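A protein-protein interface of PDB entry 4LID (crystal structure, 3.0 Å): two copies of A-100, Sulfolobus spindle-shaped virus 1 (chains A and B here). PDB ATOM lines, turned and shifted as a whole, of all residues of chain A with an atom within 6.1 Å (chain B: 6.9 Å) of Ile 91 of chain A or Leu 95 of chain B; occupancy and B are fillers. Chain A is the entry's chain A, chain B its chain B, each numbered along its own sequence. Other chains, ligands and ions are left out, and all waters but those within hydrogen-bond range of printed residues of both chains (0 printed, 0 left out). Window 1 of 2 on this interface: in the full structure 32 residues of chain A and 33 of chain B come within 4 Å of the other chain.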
ATOM      1  N   ASN A  17      -0.315  12.996  -3.157  1.00  0.00           N
ATOM      2  CA  ASN A  17      -0.733  11.781  -3.810  1.00  0.00           C
ATOM      3  C   ASN A  17      -1.745  11.109  -2.878  1.00  0.00           C
ATOM      4  O   ASN A  17      -1.543  10.998  -1.631  1.00  0.00           O
ATOM      5  CB  ASN A  17       0.456  10.888  -4.083  1.00  0.00           C
ATOM      6  CG  ASN A  17       0.062   9.613  -4.790  1.00  0.00           C
ATOM      7  OD1 ASN A  17      -0.715   9.620  -5.750  1.00  0.00           O
ATOM      8  ND2 ASN A  17       0.599   8.508  -4.324  1.00  0.00           N
ATOM      9  N   VAL A  19      -4.134   7.769  -2.472  1.00  0.00           N
ATOM     10  CA  VAL A  19      -4.520   6.470  -2.995  1.00  0.00           C
ATOM     11  C   VAL A  19      -5.545   5.850  -2.078  1.00  0.00           C
ATOM     12  O   VAL A  19      -5.320   5.634  -0.867  1.00  0.00           O
ATOM     13  CB  VAL A  19      -3.356   5.495  -3.157  1.00  0.00           C
ATOM     14  CG1 VAL A  19      -3.862   4.226  -3.816  1.00  0.00           C
ATOM     15  CG2 VAL A  19      -2.247   6.115  -4.005  1.00  0.00           C
ATOM     16  N   TYR A  21      -7.795   2.723  -1.329  1.00  0.00           N
ATOM     17  CA  TYR A  21      -7.958   1.302  -1.538  1.00  0.00           C
ATOM     18  C   TYR A  21      -9.243   0.790  -0.870  1.00  0.00           C
ATOM     19  O   TYR A  21      -9.376   0.687   0.393  1.00  0.00           O
ATOM     20  CB  TYR A  21      -6.734   0.515  -1.030  1.00  0.00           C
ATOM     21  CG  TYR A  21      -5.561   0.461  -1.983  1.00  0.00           C
ATOM     22  CD1 TYR A  21      -5.622  -0.280  -3.154  1.00  0.00           C
ATOM     23  CD2 TYR A  21      -4.390   1.149  -1.713  1.00  0.00           C
ATOM     24  CE1 TYR A  21      -4.537  -0.325  -4.024  1.00  0.00           C
ATOM     25  CE2 TYR A  21      -3.322   1.109  -2.585  1.00  0.00           C
ATOM     26  CZ  TYR A  21      -3.401   0.374  -3.722  1.00  0.00           C
ATOM     27  OH  TYR A  21      -2.333   0.301  -4.552  1.00  0.00           O
ATOM     28  N   LEU A  64       6.369  -6.394  -8.334  1.00  0.00           N
ATOM     29  CA  LEU A  64       6.749  -5.040  -8.049  1.00  0.00           C
ATOM     30  C   LEU A  64       8.196  -4.771  -8.406  1.00  0.00           C
ATOM     31  O   LEU A  64       8.531  -3.698  -8.888  1.00  0.00           O
ATOM     32  CB  LEU A  64       6.532  -4.753  -6.569  1.00  0.00           C
ATOM     33  CG  LEU A  64       5.075  -4.464  -6.189  1.00  0.00           C
ATOM     34  CD1 LEU A  64       5.027  -4.070  -4.727  1.00  0.00           C
ATOM     35  CD2 LEU A  64       4.492  -3.343  -7.004  1.00  0.00           C
ATOM     36  N   GLN A  84       2.590   2.615 -13.383  1.00  0.00           N
ATOM     37  CA  GLN A  84       2.184   3.002 -12.066  1.00  0.00           C
ATOM     38  C   GLN A  84       0.871   2.300 -11.673  1.00  0.00           C
ATOM     39  O   GLN A  84       0.713   1.805 -10.548  1.00  0.00           O
ATOM     40  CB  GLN A  84       2.008   4.505 -11.965  1.00  0.00           C
ATOM     41  CG  GLN A  84       1.374   4.846 -10.648  1.00  0.00           C
ATOM     42  CD  GLN A  84       1.128   6.293 -10.465  1.00  0.00           C
ATOM     43  OE1 GLN A  84       1.043   7.060 -11.422  1.00  0.00           O
ATOM     44  NE2 GLN A  84       1.046   6.698  -9.214  1.00  0.00           N
ATOM     45  N   GLU A  86      -0.508  -0.511 -12.855  1.00  0.00           N
ATOM     46  CA  GLU A  86      -0.249  -1.906 -12.566  1.00  0.00           C
ATOM     47  C   GLU A  86       0.333  -2.147 -11.196  1.00  0.00           C
ATOM     48  O   GLU A  86       0.006  -3.154 -10.535  1.00  0.00           O
ATOM     49  CB  GLU A  86       0.637  -2.493 -13.631  1.00  0.00           C
ATOM     50  CG  GLU A  86      -0.209  -3.060 -14.743  1.00  0.00           C
ATOM     51  CD  GLU A  86      -0.919  -4.319 -14.299  1.00  0.00           C
ATOM     52  OE1 GLU A  86      -0.503  -4.978 -13.289  1.00  0.00           O
ATOM     53  OE2 GLU A  86      -1.901  -4.640 -14.977  1.00  0.00           O
ATOM     54  N   ALA A  87       1.180  -1.220 -10.756  1.00  0.00           N
ATOM     55  CA  ALA A  87       1.815  -1.360  -9.461  1.00  0.00           C
ATOM     56  C   ALA A  87       0.724  -1.234  -8.441  1.00  0.00           C
ATOM     57  O   ALA A  87       0.618  -2.027  -7.519  1.00  0.00           O
ATOM     58  CB  ALA A  87       2.862  -0.293  -9.255  1.00  0.00           C
ATOM     59  N   LEU A  88      -0.104  -0.224  -8.624  1.00  0.00           N
ATOM     60  CA  LEU A  88      -1.185   0.015  -7.689  1.00  0.00           C
ATOM     61  C   LEU A  88      -2.064  -1.212  -7.544  1.00  0.00           C
ATOM     62  O   LEU A  88      -2.409  -1.568  -6.434  1.00  0.00           O
ATOM     63  CB  LEU A  88      -2.003   1.218  -8.103  1.00  0.00           C
ATOM     64  CG  LEU A  88      -1.255   2.541  -8.088  1.00  0.00           C
ATOM     65  CD1 LEU A  88      -2.207   3.667  -8.444  1.00  0.00           C
ATOM     66  CD2 LEU A  88      -0.604   2.826  -6.745  1.00  0.00           C
ATOM     67  N   LEU A  89      -2.393  -1.886  -8.647  1.00  0.00           N
ATOM     68  CA  LEU A  89      -3.172  -3.129  -8.543  1.00  0.00           C
ATOM     69  C   LEU A  89      -2.378  -4.186  -7.860  1.00  0.00           C
ATOM     70  O   LEU A  89      -2.889  -4.891  -7.030  1.00  0.00           O
ATOM     71  CB  LEU A  89      -3.558  -3.700  -9.888  1.00  0.00           C
ATOM     72  CG  LEU A  89      -4.880  -3.152 -10.351  1.00  0.00           C
ATOM     73  CD1 LEU A  89      -4.769  -1.660 -10.464  1.00  0.00           C
ATOM     74  CD2 LEU A  89      -5.228  -3.742 -11.684  1.00  0.00           C
ATOM     75  N   THR A  90      -1.118  -4.321  -8.220  1.00  0.00           N
ATOM     76  CA  THR A  90      -0.329  -5.323  -7.573  1.00  0.00           C
ATOM     77  C   THR A  90      -0.314  -5.065  -6.082  1.00  0.00           C
ATOM     78  O   THR A  90      -0.434  -6.009  -5.286  1.00  0.00           O
ATOM     79  CB  THR A  90       1.072  -5.337  -8.141  1.00  0.00           C
ATOM     80  OG1 THR A  90       0.978  -5.698  -9.521  1.00  0.00           O
ATOM     81  CG2 THR A  90       1.904  -6.340  -7.417  1.00  0.00           C
ATOM     82  N   ILE A  91      -0.203  -3.794  -5.694  1.00  0.00           N
ATOM     83  CA  ILE A  91      -0.215  -3.457  -4.273  1.00  0.00           C
ATOM     84  C   ILE A  91      -1.560  -3.797  -3.607  1.00  0.00           C
ATOM     85  O   ILE A  91      -1.622  -4.103  -2.422  1.00  0.00           O
ATOM     86  CB  ILE A  91       0.169  -1.999  -4.042  1.00  0.00           C
ATOM     87  CG1 ILE A  91       1.673  -1.880  -4.192  1.00  0.00           C
ATOM     88  CG2 ILE A  91      -0.245  -1.529  -2.650  1.00  0.00           C
ATOM     89  CD1 ILE A  91       2.181  -0.459  -4.141  1.00  0.00           C
ATOM     90  N   ALA A  92      -2.640  -3.756  -4.360  1.00  0.00           N
ATOM     91  CA  ALA A  92      -3.938  -4.120  -3.786  1.00  0.00           C
ATOM     92  C   ALA A  92      -3.869  -5.560  -3.321  1.00  0.00           C
ATOM     93  O   ALA A  92      -4.176  -5.886  -2.180  1.00  0.00           O
ATOM     94  CB  ALA A  92      -5.059  -3.948  -4.800  1.00  0.00           C
ATOM     95  N   LYS A  93      -3.389  -6.423  -4.188  1.00  0.00           N
ATOM     96  CA  LYS A  93      -3.334  -7.848  -3.842  1.00  0.00           C
ATOM     97  C   LYS A  93      -2.479  -8.042  -2.593  1.00  0.00           C
ATOM     98  O   LYS A  93      -2.780  -8.848  -1.732  1.00  0.00           O
ATOM     99  CB  LYS A  93      -2.787  -8.669  -4.993  1.00  0.00           C
ATOM    100  CG  LYS A  93      -3.399  -8.314  -6.336  1.00  0.00           C
ATOM    101  CD  LYS A  93      -3.066  -9.337  -7.398  1.00  0.00           C
ATOM    102  CE  LYS A  93      -2.900  -8.705  -8.773  1.00  0.00           C
ATOM    103  NZ  LYS A  93      -3.040  -9.745  -9.832  1.00  0.00           N
ATOM    104  N   ILE A  94      -1.423  -7.270  -2.474  1.00  0.00           N
ATOM    105  CA  ILE A  94      -0.564  -7.415  -1.321  1.00  0.00           C
ATOM    106  C   ILE A  94      -1.302  -7.013  -0.039  1.00  0.00           C
ATOM    107  O   ILE A  94      -1.140  -7.601   1.034  1.00  0.00           O
ATOM    108  CB  ILE A  94       0.695  -6.566  -1.511  1.00  0.00           C
ATOM    109  CG1 ILE A  94       1.578  -7.202  -2.582  1.00  0.00           C
ATOM    110  CG2 ILE A  94       1.449  -6.428  -0.203  1.00  0.00           C
ATOM    111  CD1 ILE A  94       2.790  -6.358  -2.906  1.00  0.00           C
ATOM    112  N   LEU A  95      -2.093  -5.965  -0.158  1.00  0.00           N
ATOM    113  CA  LEU A  95      -2.875  -5.512   0.966  1.00  0.00           C
ATOM    114  C   LEU A  95      -3.843  -6.620   1.367  1.00  0.00           C
ATOM    115  O   LEU A  95      -3.982  -6.918   2.567  1.00  0.00           O
ATOM    116  CB  LEU A  95      -3.622  -4.213   0.613  1.00  0.00           C
ATOM    117  CG  LEU A  95      -2.781  -2.944   0.623  1.00  0.00           C
ATOM    118  CD1 LEU A  95      -3.568  -1.749   0.142  1.00  0.00           C
ATOM    119  CD2 LEU A  95      -2.246  -2.633   2.012  1.00  0.00           C
ATOM    120  N   SER A  96      -4.484  -7.242   0.373  1.00  0.00           N
ATOM    121  CA  SER A  96      -5.493  -8.262   0.646  1.00  0.00           C
ATOM    122  C   SER A  96      -4.890  -9.387   1.499  1.00  0.00           C
ATOM    123  O   SER A  96      -5.504  -9.892   2.438  1.00  0.00           O
ATOM    124  CB  SER A  96      -6.151  -8.786  -0.638  1.00  0.00           C
ATOM    125  OG  SER A  96      -5.354  -9.722  -1.293  1.00  0.00           O
ATOM    126  N   TYR B  21      -4.505   6.244   1.577  1.00  0.00           N
ATOM    127  CA  TYR B  21      -3.154   6.764   1.592  1.00  0.00           C
ATOM    128  C   TYR B  21      -3.135   8.219   1.150  1.00  0.00           C
ATOM    129  O   TYR B  21      -3.531   8.507   0.027  1.00  0.00           O
ATOM    130  CB  TYR B  21      -2.283   5.909   0.683  1.00  0.00           C
ATOM    131  CG  TYR B  21      -1.780   4.622   1.331  1.00  0.00           C
ATOM    132  CD1 TYR B  21      -0.793   4.649   2.294  1.00  0.00           C
ATOM    133  CD2 TYR B  21      -2.260   3.386   0.938  1.00  0.00           C
ATOM    134  CE1 TYR B  21      -0.310   3.494   2.859  1.00  0.00           C
ATOM    135  CE2 TYR B  21      -1.799   2.211   1.507  1.00  0.00           C
ATOM    136  CZ  TYR B  21      -0.831   2.261   2.472  1.00  0.00           C
ATOM    137  OH  TYR B  21      -0.367   1.062   3.032  1.00  0.00           O
ATOM    138  N   LEU B  23      -0.177  10.977   0.817  1.00  0.00           N
ATOM    139  CA  LEU B  23       1.259  11.127   0.801  1.00  0.00           C
ATOM    140  C   LEU B  23       1.638  12.504   0.308  1.00  0.00           C
ATOM    141  O   LEU B  23       1.265  12.907  -0.778  1.00  0.00           O
ATOM    142  CB  LEU B  23       1.851  10.125  -0.187  1.00  0.00           C
ATOM    143  CG  LEU B  23       1.501   8.673   0.078  1.00  0.00           C
ATOM    144  CD1 LEU B  23       2.197   7.813  -0.953  1.00  0.00           C
ATOM    145  CD2 LEU B  23       1.901   8.265   1.491  1.00  0.00           C
ATOM    146  N   LEU B  57      13.347   0.642  -3.083  1.00  0.00           N
ATOM    147  CA  LEU B  57      12.348  -0.356  -3.285  1.00  0.00           C
ATOM    148  C   LEU B  57      12.803  -1.721  -2.781  1.00  0.00           C
ATOM    149  O   LEU B  57      12.087  -2.293  -1.968  1.00  0.00           O
ATOM    150  CB  LEU B  57      11.932  -0.422  -4.739  1.00  0.00           C
ATOM    151  CG  LEU B  57      10.718  -1.334  -4.934  1.00  0.00           C
ATOM    152  CD1 LEU B  57       9.455  -0.662  -4.407  1.00  0.00           C
ATOM    153  CD2 LEU B  57      10.507  -1.712  -6.384  1.00  0.00           C
ATOM    154  N   LEU B  64       8.598  -6.140   3.568  1.00  0.00           N
ATOM    155  CA  LEU B  64       7.307  -6.772   3.475  1.00  0.00           C
ATOM    156  C   LEU B  64       7.380  -8.282   3.592  1.00  0.00           C
ATOM    157  O   LEU B  64       6.506  -8.883   4.179  1.00  0.00           O
ATOM    158  CB  LEU B  64       6.635  -6.421   2.151  1.00  0.00           C
ATOM    159  CG  LEU B  64       5.938  -5.076   2.139  1.00  0.00           C
ATOM    160  CD1 LEU B  64       5.200  -4.888   0.835  1.00  0.00           C
ATOM    161  CD2 LEU B  64       4.942  -4.954   3.264  1.00  0.00           C
ATOM    162  N   LEU B  88       1.510  -1.517   6.368  1.00  0.00           N
ATOM    163  CA  LEU B  88       0.886  -0.352   5.782  1.00  0.00           C
ATOM    164  C   LEU B  88       1.888   0.789   5.623  1.00  0.00           C
ATOM    165  O   LEU B  88       1.940   1.330   4.548  1.00  0.00           O
ATOM    166  CB  LEU B  88      -0.307   0.088   6.598  1.00  0.00           C
ATOM    167  CG  LEU B  88      -1.441  -0.934   6.653  1.00  0.00           C
ATOM    168  CD1 LEU B  88      -2.605  -0.340   7.443  1.00  0.00           C
ATOM    169  CD2 LEU B  88      -1.938  -1.400   5.289  1.00  0.00           C
ATOM    170  N   THR B  90       5.104   0.544   5.381  1.00  0.00           N
ATOM    171  CA  THR B  90       6.063   0.113   4.388  1.00  0.00           C
ATOM    172  C   THR B  90       5.475   0.219   2.985  1.00  0.00           C
ATOM    173  O   THR B  90       6.137   0.609   2.016  1.00  0.00           O
ATOM    174  CB  THR B  90       6.518  -1.312   4.668  1.00  0.00           C
ATOM    175  OG1 THR B  90       7.230  -1.324   5.912  1.00  0.00           O
ATOM    176  CG2 THR B  90       7.452  -1.747   3.613  1.00  0.00           C
ATOM    177  N   ILE B  91       4.214  -0.107   2.867  1.00  0.00           N
ATOM    178  CA  ILE B  91       3.584   0.073   1.579  1.00  0.00           C
ATOM    179  C   ILE B  91       3.465   1.572   1.157  1.00  0.00           C
ATOM    180  O   ILE B  91       3.458   1.889  -0.038  1.00  0.00           O
ATOM    181  CB  ILE B  91       2.209  -0.583   1.568  1.00  0.00           C
ATOM    182  CG1 ILE B  91       2.384  -2.081   1.453  1.00  0.00           C
ATOM    183  CG2 ILE B  91       1.375  -0.074   0.414  1.00  0.00           C
ATOM    184  CD1 ILE B  91       1.090  -2.879   1.599  1.00  0.00           C
ATOM    185  N   ALA B  92       3.347   2.481   2.123  1.00  0.00           N
ATOM    186  CA  ALA B  92       3.281   3.875   1.784  1.00  0.00           C
ATOM    187  C   ALA B  92       4.563   4.209   1.051  1.00  0.00           C
ATOM    188  O   ALA B  92       4.516   4.806  -0.004  1.00  0.00           O
ATOM    189  CB  ALA B  92       3.149   4.739   3.028  1.00  0.00           C
ATOM    190  N   LYS B  93       5.703   3.797   1.591  1.00  0.00           N
ATOM    191  CA  LYS B  93       6.995   4.136   1.017  1.00  0.00           C
ATOM    192  C   LYS B  93       7.123   3.571  -0.377  1.00  0.00           C
ATOM    193  O   LYS B  93       7.770   4.155  -1.232  1.00  0.00           O
ATOM    194  CB  LYS B  93       8.141   3.569   1.847  1.00  0.00           C
ATOM    195  CG  LYS B  93       8.018   3.876   3.302  1.00  0.00           C
ATOM    196  CD  LYS B  93       9.336   3.660   3.981  1.00  0.00           C
ATOM    197  CE  LYS B  93       9.136   3.151   5.390  1.00  0.00           C
ATOM    198  NZ  LYS B  93      10.381   3.354   6.168  1.00  0.00           N
ATOM    199  N   ILE B  94       6.526   2.415  -0.597  1.00  0.00           N
ATOM    200  CA  ILE B  94       6.568   1.819  -1.916  1.00  0.00           C
ATOM    201  C   ILE B  94       5.765   2.651  -2.891  1.00  0.00           C
ATOM    202  O   ILE B  94       6.179   2.891  -4.022  1.00  0.00           O
ATOM    203  CB  ILE B  94       6.033   0.388  -1.858  1.00  0.00           C
ATOM    204  CG1 ILE B  94       7.076  -0.529  -1.182  1.00  0.00           C
ATOM    205  CG2 ILE B  94       5.705  -0.131  -3.237  1.00  0.00           C
ATOM    206  CD1 ILE B  94       6.559  -1.951  -0.944  1.00  0.00           C
ATOM    207  N   LEU B  95       4.599   3.080  -2.449  1.00  0.00           N
ATOM    208  CA  LEU B  95       3.756   3.933  -3.263  1.00  0.00           C
ATOM    209  C   LEU B  95       4.537   5.200  -3.644  1.00  0.00           C
ATOM    210  O   LEU B  95       4.541   5.600  -4.822  1.00  0.00           O
ATOM    211  CB  LEU B  95       2.471   4.280  -2.513  1.00  0.00           C
ATOM    212  CG  LEU B  95       1.416   3.161  -2.428  1.00  0.00           C
ATOM    213  CD1 LEU B  95       0.215   3.574  -1.580  1.00  0.00           C
ATOM    214  CD2 LEU B  95       0.874   2.770  -3.772  1.00  0.00           C
ATOM    215  N   SER B  96       5.223   5.803  -2.671  1.00  0.00           N
ATOM    216  CA  SER B  96       5.940   7.027  -2.951  1.00  0.00           C
ATOM    217  C   SER B  96       6.921   6.872  -4.112  1.00  0.00           C
ATOM    218  O   SER B  96       7.075   7.758  -4.960  1.00  0.00           O
ATOM    219  CB  SER B  96       6.659   7.511  -1.730  1.00  0.00           C
ATOM    220  OG  SER B  96       7.800   6.748  -1.537  1.00  0.00           O
ATOM    221  N   VAL B  97       7.523   5.717  -4.197  1.00  0.00           N
ATOM    222  CA  VAL B  97       8.421   5.427  -5.296  1.00  0.00           C
ATOM    223  C   VAL B  97       7.754   5.409  -6.674  1.00  0.00           C
ATOM    224  O   VAL B  97       8.329   5.805  -7.662  1.00  0.00           O
ATOM    225  CB  VAL B  97       9.060   4.069  -5.054  1.00  0.00           C
ATOM    226  CG1 VAL B  97       9.643   3.533  -6.321  1.00  0.00           C
ATOM    227  CG2 VAL B  97      10.122   4.229  -3.980  1.00  0.00           C
ATOM    228  N   PHE B  98       6.546   4.898  -6.750  1.00  0.00           N
ATOM    229  CA  PHE B  98       5.863   4.793  -8.032  1.00  0.00           C
ATOM    230  C   PHE B  98       5.085   6.050  -8.410  1.00  0.00           C
ATOM    231  O   PHE B  98       4.745   6.247  -9.593  1.00  0.00           O
ATOM    232  CB  PHE B  98       4.869   3.648  -7.989  1.00  0.00           C
ATOM    233  CG  PHE B  98       5.485   2.309  -8.253  1.00  0.00           C
ATOM    234  CD1 PHE B  98       5.754   1.914  -9.544  1.00  0.00           C
ATOM    235  CD2 PHE B  98       5.778   1.437  -7.202  1.00  0.00           C
ATOM    236  CE1 PHE B  98       6.318   0.680  -9.797  1.00  0.00           C
ATOM    237  CE2 PHE B  98       6.336   0.206  -7.465  1.00  0.00           C
ATOM    238  CZ  PHE B  98       6.613  -0.172  -8.761  1.00  0.00           C
ATOM    239  N   ASP B  99       4.782   6.873  -7.409  1.00  0.00           N
ATOM    240  CA  ASP B  99       3.882   7.968  -7.605  1.00  0.00           C
ATOM    241  C   ASP B  99       4.605   9.288  -7.737  1.00  0.00           C
ATOM    242  O   ASP B  99       3.936  10.285  -7.875  1.00  0.00           O
ATOM    243  CB  ASP B  99       2.899   8.039  -6.441  1.00  0.00           C
ATOM    244  CG  ASP B  99       1.988   6.739  -6.318  1.00  0.00           C
ATOM    245  OD1 ASP B  99       2.177   5.774  -7.091  1.00  0.00           O
ATOM    246  OD2 ASP B  99       1.047   6.680  -5.471  1.00  0.00           O
ATOM    247  N   PHE B 100       5.946   9.297  -7.720  1.00  0.00           N
ATOM    248  CA  PHE B 100       6.744  10.515  -7.873  1.00  0.00           C
ATOM    249  C   PHE B 100       7.933  10.308  -8.825  1.00  0.00           C
ATOM    250  O   PHE B 100       8.694   9.362  -8.663  1.00  0.00           O
ATOM    251  CB  PHE B 100       7.263  10.954  -6.518  1.00  0.00           C
ATOM    252  CG  PHE B 100       6.187  11.297  -5.487  1.00  0.00           C
ATOM    253  CD1 PHE B 100       6.532  11.486  -4.178  1.00  0.00           C
ATOM    254  CD2 PHE B 100       4.869  11.430  -5.791  1.00  0.00           C
ATOM    255  CE1 PHE B 100       5.582  11.790  -3.200  1.00  0.00           C
ATOM    256  CE2 PHE B 100       3.924  11.750  -4.817  1.00  0.00           C
ATOM    257  CZ  PHE B 100       4.275  11.929  -3.513  1.00  0.00           C
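The side-chain hydroxyl (OH) of Tyr 21 of chain A is in hydrogen-bond range of the backbone carbonyl oxygen (O) of Leu 88 of chain A (2.7 Å). OH of Tyr 21 of chain B is in hydrogen-bond range of O of Leu 88 of chain B, at 2.8 Å.
Of the printed residues of chain B, Asn 17 of chain A touches Tyr 21 (3.6 Å), Leu 23 (2.8 Å), Asp 99 (2.2 Å) and Phe 100 (3.6 Å). Printed residues of chain B within 4 Å of Gln 84 of chain A: Phe 98 (3.7 Å) and Asp 99 (2.6 Å). Of chain B, only Ile 91, Ile 94 and Leu 95 come within 4 Å of Ile 91 of chain A. Printed residues of chain A within 4 Å of Tyr 21 of chain B: Asn 17 and Val 19. Leu 95 of chain B touches two residues of chain A. Of the printed residues of chain A, Asp 99 of chain B touches Asn 17, Val 19 and Gln 84. The nearest residue of chain A that does not touch Leu 95 of chain B is Tyr 21 of chain A (4.1 Å).
Of the 16 printed residues of chain B, 10 touch a printed residue of chain A. Printed residues of chain B that touch a printed residue of chain A: Tyr 21, Leu 23, Leu 57, Leu 88, Ile 91, Ile 94, Leu 95, Phe 98, Asp 99 and Phe 100. Hydrophobic or aromatic side chains of chain B that line the printed part of chain A: Tyr 21, Leu 23, Leu 57, Leu 88, Ile 91, Ile 94, Leu 95, Phe 98 and Phe 100. Among the printed residues, 17 pairs touch across the chains. Among the printed residues, no Asp or Glu carboxylate lies within 4 Å of a Lys or Arg side-chain nitrogen of the other chain.
Among the printed residues, merely in contact across the chains: Asn 17 of chain A with Tyr 21 of chain B (3.6 Å), Asn 17 of chain A with Phe 100 of chain B (3.6 Å), Val 19 of chain A with Asp 99 of chain B (3.6 Å), Leu 64 of chain A with Leu 57 of chain B (3.8 Å), Gln 84 of chain A with Phe 98 of chain B (3.7 Å), Ala 87 of chain A with Phe 98 of chain B (3.6 Å), Leu 88 of chain A with Leu 95 of chain B (3.3 Å), Ile 91 of chain A with Ile 91 of chain B (3.8 Å), Ile 91 of chain A with Ile 94 of chain B (3.7 Å), Ile 91 of chain A with Leu 95 of chain B (3.5 Å), Ile 94 of chain A with Ile 91 of chain B (3.996 Å), Leu 95 of chain A with Leu 88 of chain B (3.5 Å) and Leu 95 of chain A with Ile 91 of chain B (3.4 Å).
Leu 88 of chain A touches Leu 95 of chain B, and with the chains exchanged Leu 95 of chain A touches Leu 88 of chain B. Ile 91 of chain B touches its own counterpart, Ile 91 of chain A. Ile 91 of chain A touches Ile 94 of chain B, and with the chains exchanged Ile 94 of chain A touches Ile 91 of chain B. Ile 91 of chain A touches Leu 95 of chain B, and with the chains exchanged Leu 95 of chain A touches Ile 91 of chain B. 10 positions are printed for both chains. Of the 17 pairs that touch across the chains among the printed residues, 7 have their exchanged pair printed and touching as well.
The backbone carbonyl oxygen (O) of Asn 17 of chain A lies within hydrogen-bond range of the backbone NH (N) of Leu 23 of chain B (2.8 Å). The side-chain carboxylate (OD2) of Asp 99 of chain B lies close to the side-chain amide oxygen (OD1) of Asn 17 of chain A (3.4 Å). O of Val 19 of chain A lies within hydrogen-bond range of N of Tyr 21 of chain B, at 2.6 Å. The side-chain amide nitrogen (NE2) of Gln 84 of chain A is in hydrogen-bond range of the side-chain carboxylate (OD1) of Asp 99 of chain B (2.6 Å).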
